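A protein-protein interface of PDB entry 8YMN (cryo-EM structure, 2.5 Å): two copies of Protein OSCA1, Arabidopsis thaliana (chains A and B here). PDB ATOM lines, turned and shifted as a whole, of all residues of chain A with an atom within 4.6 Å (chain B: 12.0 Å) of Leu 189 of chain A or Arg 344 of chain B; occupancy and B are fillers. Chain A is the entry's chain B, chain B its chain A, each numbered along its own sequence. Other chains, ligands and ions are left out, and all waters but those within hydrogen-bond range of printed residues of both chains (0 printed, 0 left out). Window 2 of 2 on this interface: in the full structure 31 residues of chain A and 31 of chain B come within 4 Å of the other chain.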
ATOM      1  N   ALA A 185      19.733  13.045  17.522  1.00  0.00           N
ATOM      2  CA  ALA A 185      18.771  13.636  16.601  1.00  0.00           C
ATOM      3  C   ALA A 185      18.502  12.722  15.426  1.00  0.00           C
ATOM      4  O   ALA A 185      17.363  12.561  15.019  1.00  0.00           O
ATOM      5  CB  ALA A 185      19.265  14.985  16.117  1.00  0.00           C
ATOM      6  N   ASN A 186      19.547  12.115  14.884  1.00  0.00           N
ATOM      7  CA  ASN A 186      19.393  11.212  13.756  1.00  0.00           C
ATOM      8  C   ASN A 186      18.673   9.961  14.190  1.00  0.00           C
ATOM      9  O   ASN A 186      17.915   9.387  13.420  1.00  0.00           O
ATOM     10  CB  ASN A 186      20.754  10.867  13.162  1.00  0.00           C
ATOM     11  CG  ASN A 186      21.411  12.049  12.486  1.00  0.00           C
ATOM     12  OD1 ASN A 186      20.737  12.977  12.041  1.00  0.00           O
ATOM     13  ND2 ASN A 186      22.733  12.024  12.407  1.00  0.00           N
ATOM     14  N   MET A 187      18.893   9.540  15.426  1.00  0.00           N
ATOM     15  CA  MET A 187      18.210   8.376  15.958  1.00  0.00           C
ATOM     16  C   MET A 187      16.741   8.679  16.140  1.00  0.00           C
ATOM     17  O   MET A 187      15.900   7.841  15.847  1.00  0.00           O
ATOM     18  CB  MET A 187      18.823   7.981  17.294  1.00  0.00           C
ATOM     19  CG  MET A 187      19.586   6.669  17.272  1.00  0.00           C
ATOM     20  SD  MET A 187      20.249   6.236  18.890  1.00  0.00           S
ATOM     21  CE  MET A 187      21.314   7.636  19.189  1.00  0.00           C
ATOM     22  N   ARG A 188      16.426   9.875  16.617  1.00  0.00           N
ATOM     23  CA  ARG A 188      15.041  10.270  16.818  1.00  0.00           C
ATOM     24  C   ARG A 188      14.315  10.346  15.499  1.00  0.00           C
ATOM     25  O   ARG A 188      13.176   9.917  15.393  1.00  0.00           O
ATOM     26  CB  ARG A 188      14.976  11.608  17.556  1.00  0.00           C
ATOM     27  CG  ARG A 188      13.883  12.553  17.099  1.00  0.00           C
ATOM     28  CD  ARG A 188      13.563  13.568  18.173  1.00  0.00           C
ATOM     29  NE  ARG A 188      12.272  14.203  17.956  1.00  0.00           N
ATOM     30  CZ  ARG A 188      11.258  14.138  18.808  1.00  0.00           C
ATOM     31  NH1 ARG A 188      11.387  13.462  19.935  1.00  0.00           N
ATOM     32  NH2 ARG A 188      10.116  14.748  18.532  1.00  0.00           N
ATOM     33  N   LEU A 189      14.980  10.863  14.477  1.00  0.00           N
ATOM     34  CA  LEU A 189      14.355  11.008  13.181  1.00  0.00           C
ATOM     35  C   LEU A 189      14.175   9.660  12.519  1.00  0.00           C
ATOM     36  O   LEU A 189      13.161   9.425  11.872  1.00  0.00           O
ATOM     37  CB  LEU A 189      15.173  11.955  12.313  1.00  0.00           C
ATOM     38  CG  LEU A 189      15.040  13.434  12.677  1.00  0.00           C
ATOM     39  CD1 LEU A 189      16.146  14.250  12.030  1.00  0.00           C
ATOM     40  CD2 LEU A 189      13.671  13.965  12.286  1.00  0.00           C
ATOM     41  N   GLN A 190      15.142   8.765  12.688  1.00  0.00           N
ATOM     42  CA  GLN A 190      15.017   7.418  12.147  1.00  0.00           C
ATOM     43  C   GLN A 190      13.889   6.694  12.852  1.00  0.00           C
ATOM     44  O   GLN A 190      13.117   5.977  12.224  1.00  0.00           O
ATOM     45  CB  GLN A 190      16.346   6.667  12.287  1.00  0.00           C
ATOM     46  CG  GLN A 190      16.264   5.259  12.865  1.00  0.00           C
ATOM     47  CD  GLN A 190      17.089   5.091  14.132  1.00  0.00           C
ATOM     48  OE1 GLN A 190      18.318   5.157  14.098  1.00  0.00           O
ATOM     49  NE2 GLN A 190      16.415   4.871  15.256  1.00  0.00           N
ATOM     50  N   PHE A 191      13.761   6.911  14.152  1.00  0.00           N
ATOM     51  CA  PHE A 191      12.720   6.261  14.924  1.00  0.00           C
ATOM     52  C   PHE A 191      11.362   6.789  14.537  1.00  0.00           C
ATOM     53  O   PHE A 191      10.430   6.021  14.364  1.00  0.00           O
ATOM     54  CB  PHE A 191      12.960   6.497  16.414  1.00  0.00           C
ATOM     55  CG  PHE A 191      12.054   5.714  17.308  1.00  0.00           C
ATOM     56  CD1 PHE A 191      12.279   4.371  17.534  1.00  0.00           C
ATOM     57  CD2 PHE A 191      10.979   6.322  17.926  1.00  0.00           C
ATOM     58  CE1 PHE A 191      11.447   3.644  18.358  1.00  0.00           C
ATOM     59  CE2 PHE A 191      10.142   5.602  18.746  1.00  0.00           C
ATOM     60  CZ  PHE A 191      10.375   4.261  18.965  1.00  0.00           C
ATOM     61  N   LEU A 192      11.247   8.100  14.391  1.00  0.00           N
ATOM     62  CA  LEU A 192       9.970   8.712  14.064  1.00  0.00           C
ATOM     63  C   LEU A 192       9.500   8.339  12.678  1.00  0.00           C
ATOM     64  O   LEU A 192       8.308   8.328  12.420  1.00  0.00           O
ATOM     65  CB  LEU A 192      10.076  10.228  14.175  1.00  0.00           C
ATOM     66  CG  LEU A 192       9.366  10.907  15.343  1.00  0.00           C
ATOM     67  CD1 LEU A 192       9.111   9.929  16.477  1.00  0.00           C
ATOM     68  CD2 LEU A 192      10.188  12.090  15.820  1.00  0.00           C
ATOM     69  N   ALA A 193      10.432   8.033  11.786  1.00  0.00           N
ATOM     70  CA  ALA A 193      10.084   7.664  10.426  1.00  0.00           C
ATOM     71  C   ALA A 193       9.680   6.213  10.340  1.00  0.00           C
ATOM     72  O   ALA A 193       8.804   5.857   9.559  1.00  0.00           O
ATOM     73  CB  ALA A 193      11.255   7.924   9.506  1.00  0.00           C
ATOM     74  N   ARG A 676      20.758  24.057  15.389  1.00  0.00           N
ATOM     75  CA  ARG A 676      21.053  23.007  14.436  1.00  0.00           C
ATOM     76  C   ARG A 676      20.405  21.697  14.799  1.00  0.00           C
ATOM     77  O   ARG A 676      19.885  21.003  13.930  1.00  0.00           O
ATOM     78  CB  ARG A 676      22.561  22.802  14.310  1.00  0.00           C
ATOM     79  CG  ARG A 676      23.080  22.894  12.887  1.00  0.00           C
ATOM     80  CD  ARG A 676      23.473  21.530  12.350  1.00  0.00           C
ATOM     81  NE  ARG A 676      22.310  20.681  12.116  1.00  0.00           N
ATOM     82  CZ  ARG A 676      22.353  19.506  11.500  1.00  0.00           C
ATOM     83  NH1 ARG A 676      23.506  19.033  11.050  1.00  0.00           N
ATOM     84  NH2 ARG A 676      21.244  18.802  11.336  1.00  0.00           N
ATOM     85  N   ALA A 680      14.899  19.484  15.806  1.00  0.00           N
ATOM     86  CA  ALA A 680      14.482  18.114  15.523  1.00  0.00           C
ATOM     87  C   ALA A 680      13.694  17.498  16.658  1.00  0.00           C
ATOM     88  O   ALA A 680      12.884  16.605  16.436  1.00  0.00           O
ATOM     89  CB  ALA A 680      15.699  17.257  15.226  1.00  0.00           C
ATOM     90  N   PRO A 685       9.719  18.019  11.112  1.00  0.00           N
ATOM     91  CA  PRO A 685       9.914  18.603   9.787  1.00  0.00           C
ATOM     92  C   PRO A 685       8.817  18.185   8.825  1.00  0.00           C
ATOM     93  O   PRO A 685       8.386  17.039   8.855  1.00  0.00           O
ATOM     94  CB  PRO A 685      11.274  18.057   9.350  1.00  0.00           C
ATOM     95  CG  PRO A 685      11.634  16.988  10.323  1.00  0.00           C
ATOM     96  CD  PRO A 685      10.910  17.300  11.587  1.00  0.00           C
ATOM     97  N   GLU A 688       9.717  15.285   6.409  1.00  0.00           N
ATOM     98  CA  GLU A 688       9.688  13.991   7.064  1.00  0.00           C
ATOM     99  C   GLU A 688       8.262  13.532   7.252  1.00  0.00           C
ATOM    100  O   GLU A 688       7.960  12.358   7.076  1.00  0.00           O
ATOM    101  CB  GLU A 688      10.392  14.101   8.409  1.00  0.00           C
ATOM    102  CG  GLU A 688      11.383  12.989   8.687  1.00  0.00           C
ATOM    103  CD  GLU A 688      12.789  13.352   8.268  1.00  0.00           C
ATOM    104  OE1 GLU A 688      13.690  12.498   8.401  1.00  0.00           O
ATOM    105  OE2 GLU A 688      12.994  14.491   7.804  1.00  0.00           O
ATOM    106  N   ARG B 207      15.787  30.056   1.806  1.00  0.00           N
ATOM    107  CA  ARG B 207      17.220  30.272   1.794  1.00  0.00           C
ATOM    108  C   ARG B 207      17.950  28.978   2.039  1.00  0.00           C
ATOM    109  O   ARG B 207      17.341  28.004   2.465  1.00  0.00           O
ATOM    110  CB  ARG B 207      17.612  31.306   2.844  1.00  0.00           C
ATOM    111  CG  ARG B 207      17.330  32.741   2.440  1.00  0.00           C
ATOM    112  CD  ARG B 207      17.971  33.715   3.412  1.00  0.00           C
ATOM    113  NE  ARG B 207      18.738  34.747   2.722  1.00  0.00           N
ATOM    114  CZ  ARG B 207      20.058  34.720   2.564  1.00  0.00           C
ATOM    115  NH1 ARG B 207      20.766  33.710   3.049  1.00  0.00           N
ATOM    116  NH2 ARG B 207      20.670  35.703   1.921  1.00  0.00           N
ATOM    117  N   ASN B 208      19.250  28.963   1.778  1.00  0.00           N
ATOM    118  CA  ASN B 208      20.062  27.760   1.944  1.00  0.00           C
ATOM    119  C   ASN B 208      19.474  26.524   1.307  1.00  0.00           C
ATOM    120  O   ASN B 208      19.326  25.503   1.964  1.00  0.00           O
ATOM    121  CB  ASN B 208      20.429  27.509   3.406  1.00  0.00           C
ATOM    122  CG  ASN B 208      21.855  27.026   3.569  1.00  0.00           C
ATOM    123  OD1 ASN B 208      22.627  27.003   2.611  1.00  0.00           O
ATOM    124  ND2 ASN B 208      22.214  26.636   4.784  1.00  0.00           N
ATOM    125  N   PRO B 210      19.830  23.331  -0.334  1.00  0.00           N
ATOM    126  CA  PRO B 210      21.004  22.459  -0.413  1.00  0.00           C
ATOM    127  C   PRO B 210      21.457  22.171  -1.837  1.00  0.00           C
ATOM    128  O   PRO B 210      20.643  21.784  -2.671  1.00  0.00           O
ATOM    129  CB  PRO B 210      20.539  21.177   0.279  1.00  0.00           C
ATOM    130  CG  PRO B 210      19.056  21.253   0.312  1.00  0.00           C
ATOM    131  CD  PRO B 210      18.737  22.708   0.420  1.00  0.00           C
ATOM    132  N   PHE B 224      10.851  20.299  -4.458  1.00  0.00           N
ATOM    133  CA  PHE B 224      10.662  20.270  -3.019  1.00  0.00           C
ATOM    134  C   PHE B 224       9.286  20.763  -2.666  1.00  0.00           C
ATOM    135  O   PHE B 224       8.583  20.136  -1.896  1.00  0.00           O
ATOM    136  CB  PHE B 224      11.694  21.150  -2.324  1.00  0.00           C
ATOM    137  CG  PHE B 224      11.653  21.071  -0.825  1.00  0.00           C
ATOM    138  CD1 PHE B 224      12.322  20.065  -0.157  1.00  0.00           C
ATOM    139  CD2 PHE B 224      10.955  22.010  -0.085  1.00  0.00           C
ATOM    140  CE1 PHE B 224      12.292  19.989   1.220  1.00  0.00           C
ATOM    141  CE2 PHE B 224      10.917  21.939   1.290  1.00  0.00           C
ATOM    142  CZ  PHE B 224      11.587  20.927   1.944  1.00  0.00           C
ATOM    143  N   ASN B 228       6.270  18.795  -0.865  1.00  0.00           N
ATOM    144  CA  ASN B 228       6.080  19.167   0.528  1.00  0.00           C
ATOM    145  C   ASN B 228       4.915  20.116   0.683  1.00  0.00           C
ATOM    146  O   ASN B 228       4.264  20.124   1.723  1.00  0.00           O
ATOM    147  CB  ASN B 228       7.352  19.767   1.110  1.00  0.00           C
ATOM    148  CG  ASN B 228       8.394  18.719   1.430  1.00  0.00           C
ATOM    149  OD1 ASN B 228       9.180  18.326   0.574  1.00  0.00           O
ATOM    150  ND2 ASN B 228       8.406  18.265   2.674  1.00  0.00           N
ATOM    151  N   HIS B 229       4.644  20.922  -0.335  1.00  0.00           N
ATOM    152  CA  HIS B 229       3.481  21.805  -0.304  1.00  0.00           C
ATOM    153  C   HIS B 229       2.737  21.610  -1.605  1.00  0.00           C
ATOM    154  O   HIS B 229       2.546  22.560  -2.351  1.00  0.00           O
ATOM    155  CB  HIS B 229       3.913  23.260  -0.159  1.00  0.00           C
ATOM    156  CG  HIS B 229       4.610  23.558   1.131  1.00  0.00           C
ATOM    157  ND1 HIS B 229       3.943  24.002   2.252  1.00  0.00           N
ATOM    158  CD2 HIS B 229       5.915  23.474   1.479  1.00  0.00           C
ATOM    159  CE1 HIS B 229       4.807  24.178   3.235  1.00  0.00           C
ATOM    160  NE2 HIS B 229       6.010  23.865   2.792  1.00  0.00           N
ATOM    161  N   THR B 340       6.842  27.164   9.387  1.00  0.00           N
ATOM    162  CA  THR B 340       6.990  25.722   9.536  1.00  0.00           C
ATOM    163  C   THR B 340       8.403  25.280   9.177  1.00  0.00           C
ATOM    164  O   THR B 340       9.051  25.896   8.334  1.00  0.00           O
ATOM    165  CB  THR B 340       5.908  24.976   8.716  1.00  0.00           C
ATOM    166  OG1 THR B 340       5.098  24.183   9.591  1.00  0.00           O
ATOM    167  CG2 THR B 340       6.497  24.096   7.631  1.00  0.00           C
ATOM    168  N   THR B 341       8.914  24.254   9.853  1.00  0.00           N
ATOM    169  CA  THR B 341      10.228  23.719   9.508  1.00  0.00           C
ATOM    170  C   THR B 341      10.033  22.760   8.358  1.00  0.00           C
ATOM    171  O   THR B 341       9.108  21.955   8.369  1.00  0.00           O
ATOM    172  CB  THR B 341      10.925  23.029  10.693  1.00  0.00           C
ATOM    173  OG1 THR B 341      11.896  22.096  10.203  1.00  0.00           O
ATOM    174  CG2 THR B 341       9.918  22.301  11.563  1.00  0.00           C
ATOM    175  N   GLN B 342      10.890  22.837   7.357  1.00  0.00           N
ATOM    176  CA  GLN B 342      10.695  22.027   6.168  1.00  0.00           C
ATOM    177  C   GLN B 342      11.484  20.743   6.126  1.00  0.00           C
ATOM    178  O   GLN B 342      11.026  19.762   5.553  1.00  0.00           O
ATOM    179  CB  GLN B 342      11.043  22.865   4.942  1.00  0.00           C
ATOM    180  CG  GLN B 342      10.580  24.304   5.023  1.00  0.00           C
ATOM    181  CD  GLN B 342       9.119  24.452   4.674  1.00  0.00           C
ATOM    182  OE1 GLN B 342       8.589  23.705   3.858  1.00  0.00           O
ATOM    183  NE2 GLN B 342       8.461  25.416   5.293  1.00  0.00           N
ATOM    184  N   THR B 343      12.667  20.737   6.722  1.00  0.00           N
ATOM    185  CA  THR B 343      13.521  19.565   6.631  1.00  0.00           C
ATOM    186  C   THR B 343      14.216  19.246   7.943  1.00  0.00           C
ATOM    187  O   THR B 343      14.216  20.065   8.855  1.00  0.00           O
ATOM    188  CB  THR B 343      14.545  19.741   5.487  1.00  0.00           C
ATOM    189  OG1 THR B 343      15.523  18.695   5.528  1.00  0.00           O
ATOM    190  CG2 THR B 343      15.241  21.073   5.601  1.00  0.00           C
ATOM    191  N   ARG B 344      14.783  18.045   8.057  1.00  0.00           N
ATOM    192  CA  ARG B 344      15.491  17.632   9.266  1.00  0.00           C
ATOM    193  C   ARG B 344      16.640  18.558   9.617  1.00  0.00           C
ATOM    194  O   ARG B 344      16.958  18.695  10.793  1.00  0.00           O
ATOM    195  CB  ARG B 344      15.993  16.200   9.122  1.00  0.00           C
ATOM    196  CG  ARG B 344      16.541  15.857   7.751  1.00  0.00           C
ATOM    197  CD  ARG B 344      17.217  14.502   7.775  1.00  0.00           C
ATOM    198  NE  ARG B 344      16.259  13.427   8.011  1.00  0.00           N
ATOM    199  CZ  ARG B 344      16.491  12.377   8.790  1.00  0.00           C
ATOM    200  NH1 ARG B 344      17.655  12.258   9.414  1.00  0.00           N
ATOM    201  NH2 ARG B 344      15.561  11.446   8.945  1.00  0.00           N
ATOM    202  N   ASN B 345      17.286  19.167   8.623  1.00  0.00           N
ATOM    203  CA  ASN B 345      18.323  20.152   8.895  1.00  0.00           C
ATOM    204  C   ASN B 345      17.626  21.488   8.972  1.00  0.00           C
ATOM    205  O   ASN B 345      17.201  22.020   7.959  1.00  0.00           O
ATOM    206  CB  ASN B 345      19.351  20.175   7.771  1.00  0.00           C
ATOM    207  CG  ASN B 345      20.655  20.831   8.179  1.00  0.00           C
ATOM    208  OD1 ASN B 345      20.718  21.569   9.159  1.00  0.00           O
ATOM    209  ND2 ASN B 345      21.708  20.566   7.420  1.00  0.00           N
ATOM    210  N   PRO B 346      17.515  22.054  10.177  1.00  0.00           N
ATOM    211  CA  PRO B 346      16.749  23.295  10.299  1.00  0.00           C
ATOM    212  C   PRO B 346      17.497  24.510   9.772  1.00  0.00           C
ATOM    213  O   PRO B 346      16.953  25.608   9.808  1.00  0.00           O
ATOM    214  CB  PRO B 346      16.524  23.405  11.803  1.00  0.00           C
ATOM    215  CG  PRO B 346      17.713  22.737  12.405  1.00  0.00           C
ATOM    216  CD  PRO B 346      18.144  21.660  11.450  1.00  0.00           C
ATOM    217  N   THR B 347      18.717  24.319   9.285  1.00  0.00           N
ATOM    218  CA  THR B 347      19.499  25.413   8.738  1.00  0.00           C
ATOM    219  C   THR B 347      19.461  25.373   7.223  1.00  0.00           C
ATOM    220  O   THR B 347      20.073  26.205   6.568  1.00  0.00           O
ATOM    221  CB  THR B 347      20.960  25.338   9.207  1.00  0.00           C
ATOM    222  OG1 THR B 347      21.672  24.382   8.412  1.00  0.00           O
ATOM    223  CG2 THR B 347      21.030  24.927  10.669  1.00  0.00           C
ATOM    224  N   GLU B 348      18.755  24.401   6.661  1.00  0.00           N
ATOM    225  CA  GLU B 348      18.616  24.315   5.220  1.00  0.00           C
ATOM    226  C   GLU B 348      17.159  24.519   4.909  1.00  0.00           C
ATOM    227  O   GLU B 348      16.324  24.349   5.794  1.00  0.00           O
ATOM    228  CB  GLU B 348      19.069  22.957   4.719  1.00  0.00           C
ATOM    229  CG  GLU B 348      20.511  22.919   4.259  1.00  0.00           C
ATOM    230  CD  GLU B 348      21.057  21.512   4.207  1.00  0.00           C
ATOM    231  OE1 GLU B 348      20.247  20.562   4.214  1.00  0.00           O
ATOM    232  OE2 GLU B 348      22.292  21.352   4.164  1.00  0.00           O
ATOM    233  N   TRP B 349      16.839  24.884   3.672  1.00  0.00           N
ATOM    234  CA  TRP B 349      15.457  25.168   3.292  1.00  0.00           C
ATOM    235  C   TRP B 349      14.787  26.102   4.283  1.00  0.00           C
ATOM    236  O   TRP B 349      13.665  25.852   4.705  1.00  0.00           O
ATOM    237  CB  TRP B 349      14.631  23.886   3.151  1.00  0.00           C
ATOM    238  CG  TRP B 349      15.012  22.993   2.013  1.00  0.00           C
ATOM    239  CD1 TRP B 349      15.642  21.790   2.098  1.00  0.00           C
ATOM    240  CD2 TRP B 349      14.764  23.216   0.620  1.00  0.00           C
ATOM    241  NE1 TRP B 349      15.805  21.249   0.851  1.00  0.00           N
ATOM    242  CE2 TRP B 349      15.281  22.109  -0.077  1.00  0.00           C
ATOM    243  CE3 TRP B 349      14.159  24.242  -0.104  1.00  0.00           C
ATOM    244  CZ2 TRP B 349      15.214  22.003  -1.462  1.00  0.00           C
ATOM    245  CZ3 TRP B 349      14.095  24.136  -1.474  1.00  0.00           C
ATOM    246  CH2 TRP B 349      14.619  23.026  -2.139  1.00  0.00           C
ATOM    247  N   LEU B 350      15.467  27.179   4.655  1.00  0.00           N
ATOM    248  CA  LEU B 350      14.909  28.134   5.598  1.00  0.00           C
ATOM    249  C   LEU B 350      13.882  29.007   4.925  1.00  0.00           C
ATOM    250  O   LEU B 350      14.211  29.762   4.030  1.00  0.00           O
ATOM    251  CB  LEU B 350      16.000  29.024   6.172  1.00  0.00           C
ATOM    252  CG  LEU B 350      17.289  28.416   6.701  1.00  0.00           C
ATOM    253  CD1 LEU B 350      18.447  29.110   6.013  1.00  0.00           C
ATOM    254  CD2 LEU B 350      17.360  28.639   8.200  1.00  0.00           C
ATOM    255  N   THR B 351      12.639  28.930   5.370  1.00  0.00           N
ATOM    256  CA  THR B 351      11.575  29.695   4.741  1.00  0.00           C
ATOM    257  C   THR B 351      11.080  30.819   5.631  1.00  0.00           C
ATOM    258  O   THR B 351      10.742  30.592   6.783  1.00  0.00           O
ATOM    259  CB  THR B 351      10.406  28.785   4.356  1.00  0.00           C
ATOM    260  OG1 THR B 351      10.098  27.926   5.457  1.00  0.00           O
ATOM    261  CG2 THR B 351      10.777  27.935   3.163  1.00  0.00           C
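Of the 13 printed residues of chain A, 4 touch a printed residue of chain B.
Hydrophobic or aromatic side chains of chain A that line the printed part of chain B: Leu 189 and Pro 685.
Of the 18 printed residues of chain B, 6 touch a printed residue of chain A.
Printed residues of chain B that touch a printed residue of chain A: Thr 341, Thr 343, Arg 344, Asn 345, Pro 346 and Thr 347.
Hydrophobic or aromatic side chains of chain B that line the printed part of chain A: Pro 346.
Among the printed residues, 8 pairs touch across the chains.
Among the printed residues, Asp or Glu carboxylates within 4 Å of a Lys or Arg side-chain nitrogen of the other chain: Glu 688 of chain A with Arg 344 of chain B (2.2 Å).
No position is printed for both chains.
Of chain B, only Arg 344 comes within 4 Å of Leu 189 of chain A.
Of chain A, only Leu 189 (3.4 Å), Pro 685 (3.7 Å) and Glu 688 (2.2 Å) come within 4 Å of Arg 344 of chain B.
No residue of chain B comes within 4 Å of Ala 185 of chain A.
No residue of chain B comes within 4 Å of Arg 188 of chain A.
No residue of chain B comes within 4 Å of Gln 190 of chain A.
No residue of chain B comes within 4 Å of Leu 192 of chain A.
No residue of chain B comes within 4 Å of Ala 193 of chain A.
No residue of chain B comes within 4 Å of Ala 680 of chain A.
Of the printed residues of chain B, Pro 685 of chain A touches Thr 341, Thr 343 and Arg 344.
Glu 688 of chain A touches just one residue of chain B: Arg 344.
Of the printed residues of chain A, Thr 343 of chain B touches Pro 685.
Of the printed residues of chain B, Arg 676 of chain A touches Asn 345 (3.5 Å), Pro 346 (3.1 Å) and Thr 347 (3.6 Å).
Printed residues of chain A within 4 Å of Thr 347 of chain B: Arg 676 (3.6 Å).
Printed residues of chain A within 4 Å of Thr 341 of chain B: Pro 685 (3.7 Å).
The nearest printed residue of chain A that does not touch Thr 347 of chain B is Ala 680 of chain A (9.0 Å).
O of Thr 347 of chain B sits at hydrogen-bond distance from ND2 of Asn 208 of chain B (2.8 Å).
The side-chain hydroxyl (OG1) of Thr 341 of chain B sits at hydrogen-bond distance from the backbone carbonyl oxygen (O) of Thr 343 of chain B (3.4 Å).
OD1 of Asn 345 of chain B sits at hydrogen-bond distance from OG1 of Thr 347 of chain B (3.1 Å).
The side-chain carboxylate (OE2) of Glu 348 of chain B is in hydrogen-bond range of the side-chain amide nitrogen (ND2) of Asn 345 of chain B.
The guanidinium group (NE) of Arg 344 of chain B is in salt-bridge range of the side-chain carboxylate (OE1) of Glu 688 of chain A (2.8 Å).
OD1 of Asn 345 of chain B is in hydrogen-bond range of NE of Arg 676 of chain A, at 3.5 Å.
Arg 344 of chain B touches Leu 189 of chain A.
O of Arg 676 of chain A touches CD of Pro 346 of chain B, 3.1 Å away.
CG of Arg 676 of chain A touches CG2 of Thr 347 of chain B (3.6 Å).
Pro 685 of chain A touches Thr 341 of chain B (CA to O, 3.7 Å).
Pro 685 of chain A touches Thr 343 of chain B (CB to C, 3.5 Å).
CB of Pro 685 of chain A touches N of Arg 344 of chain B, at 3.7 Å.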
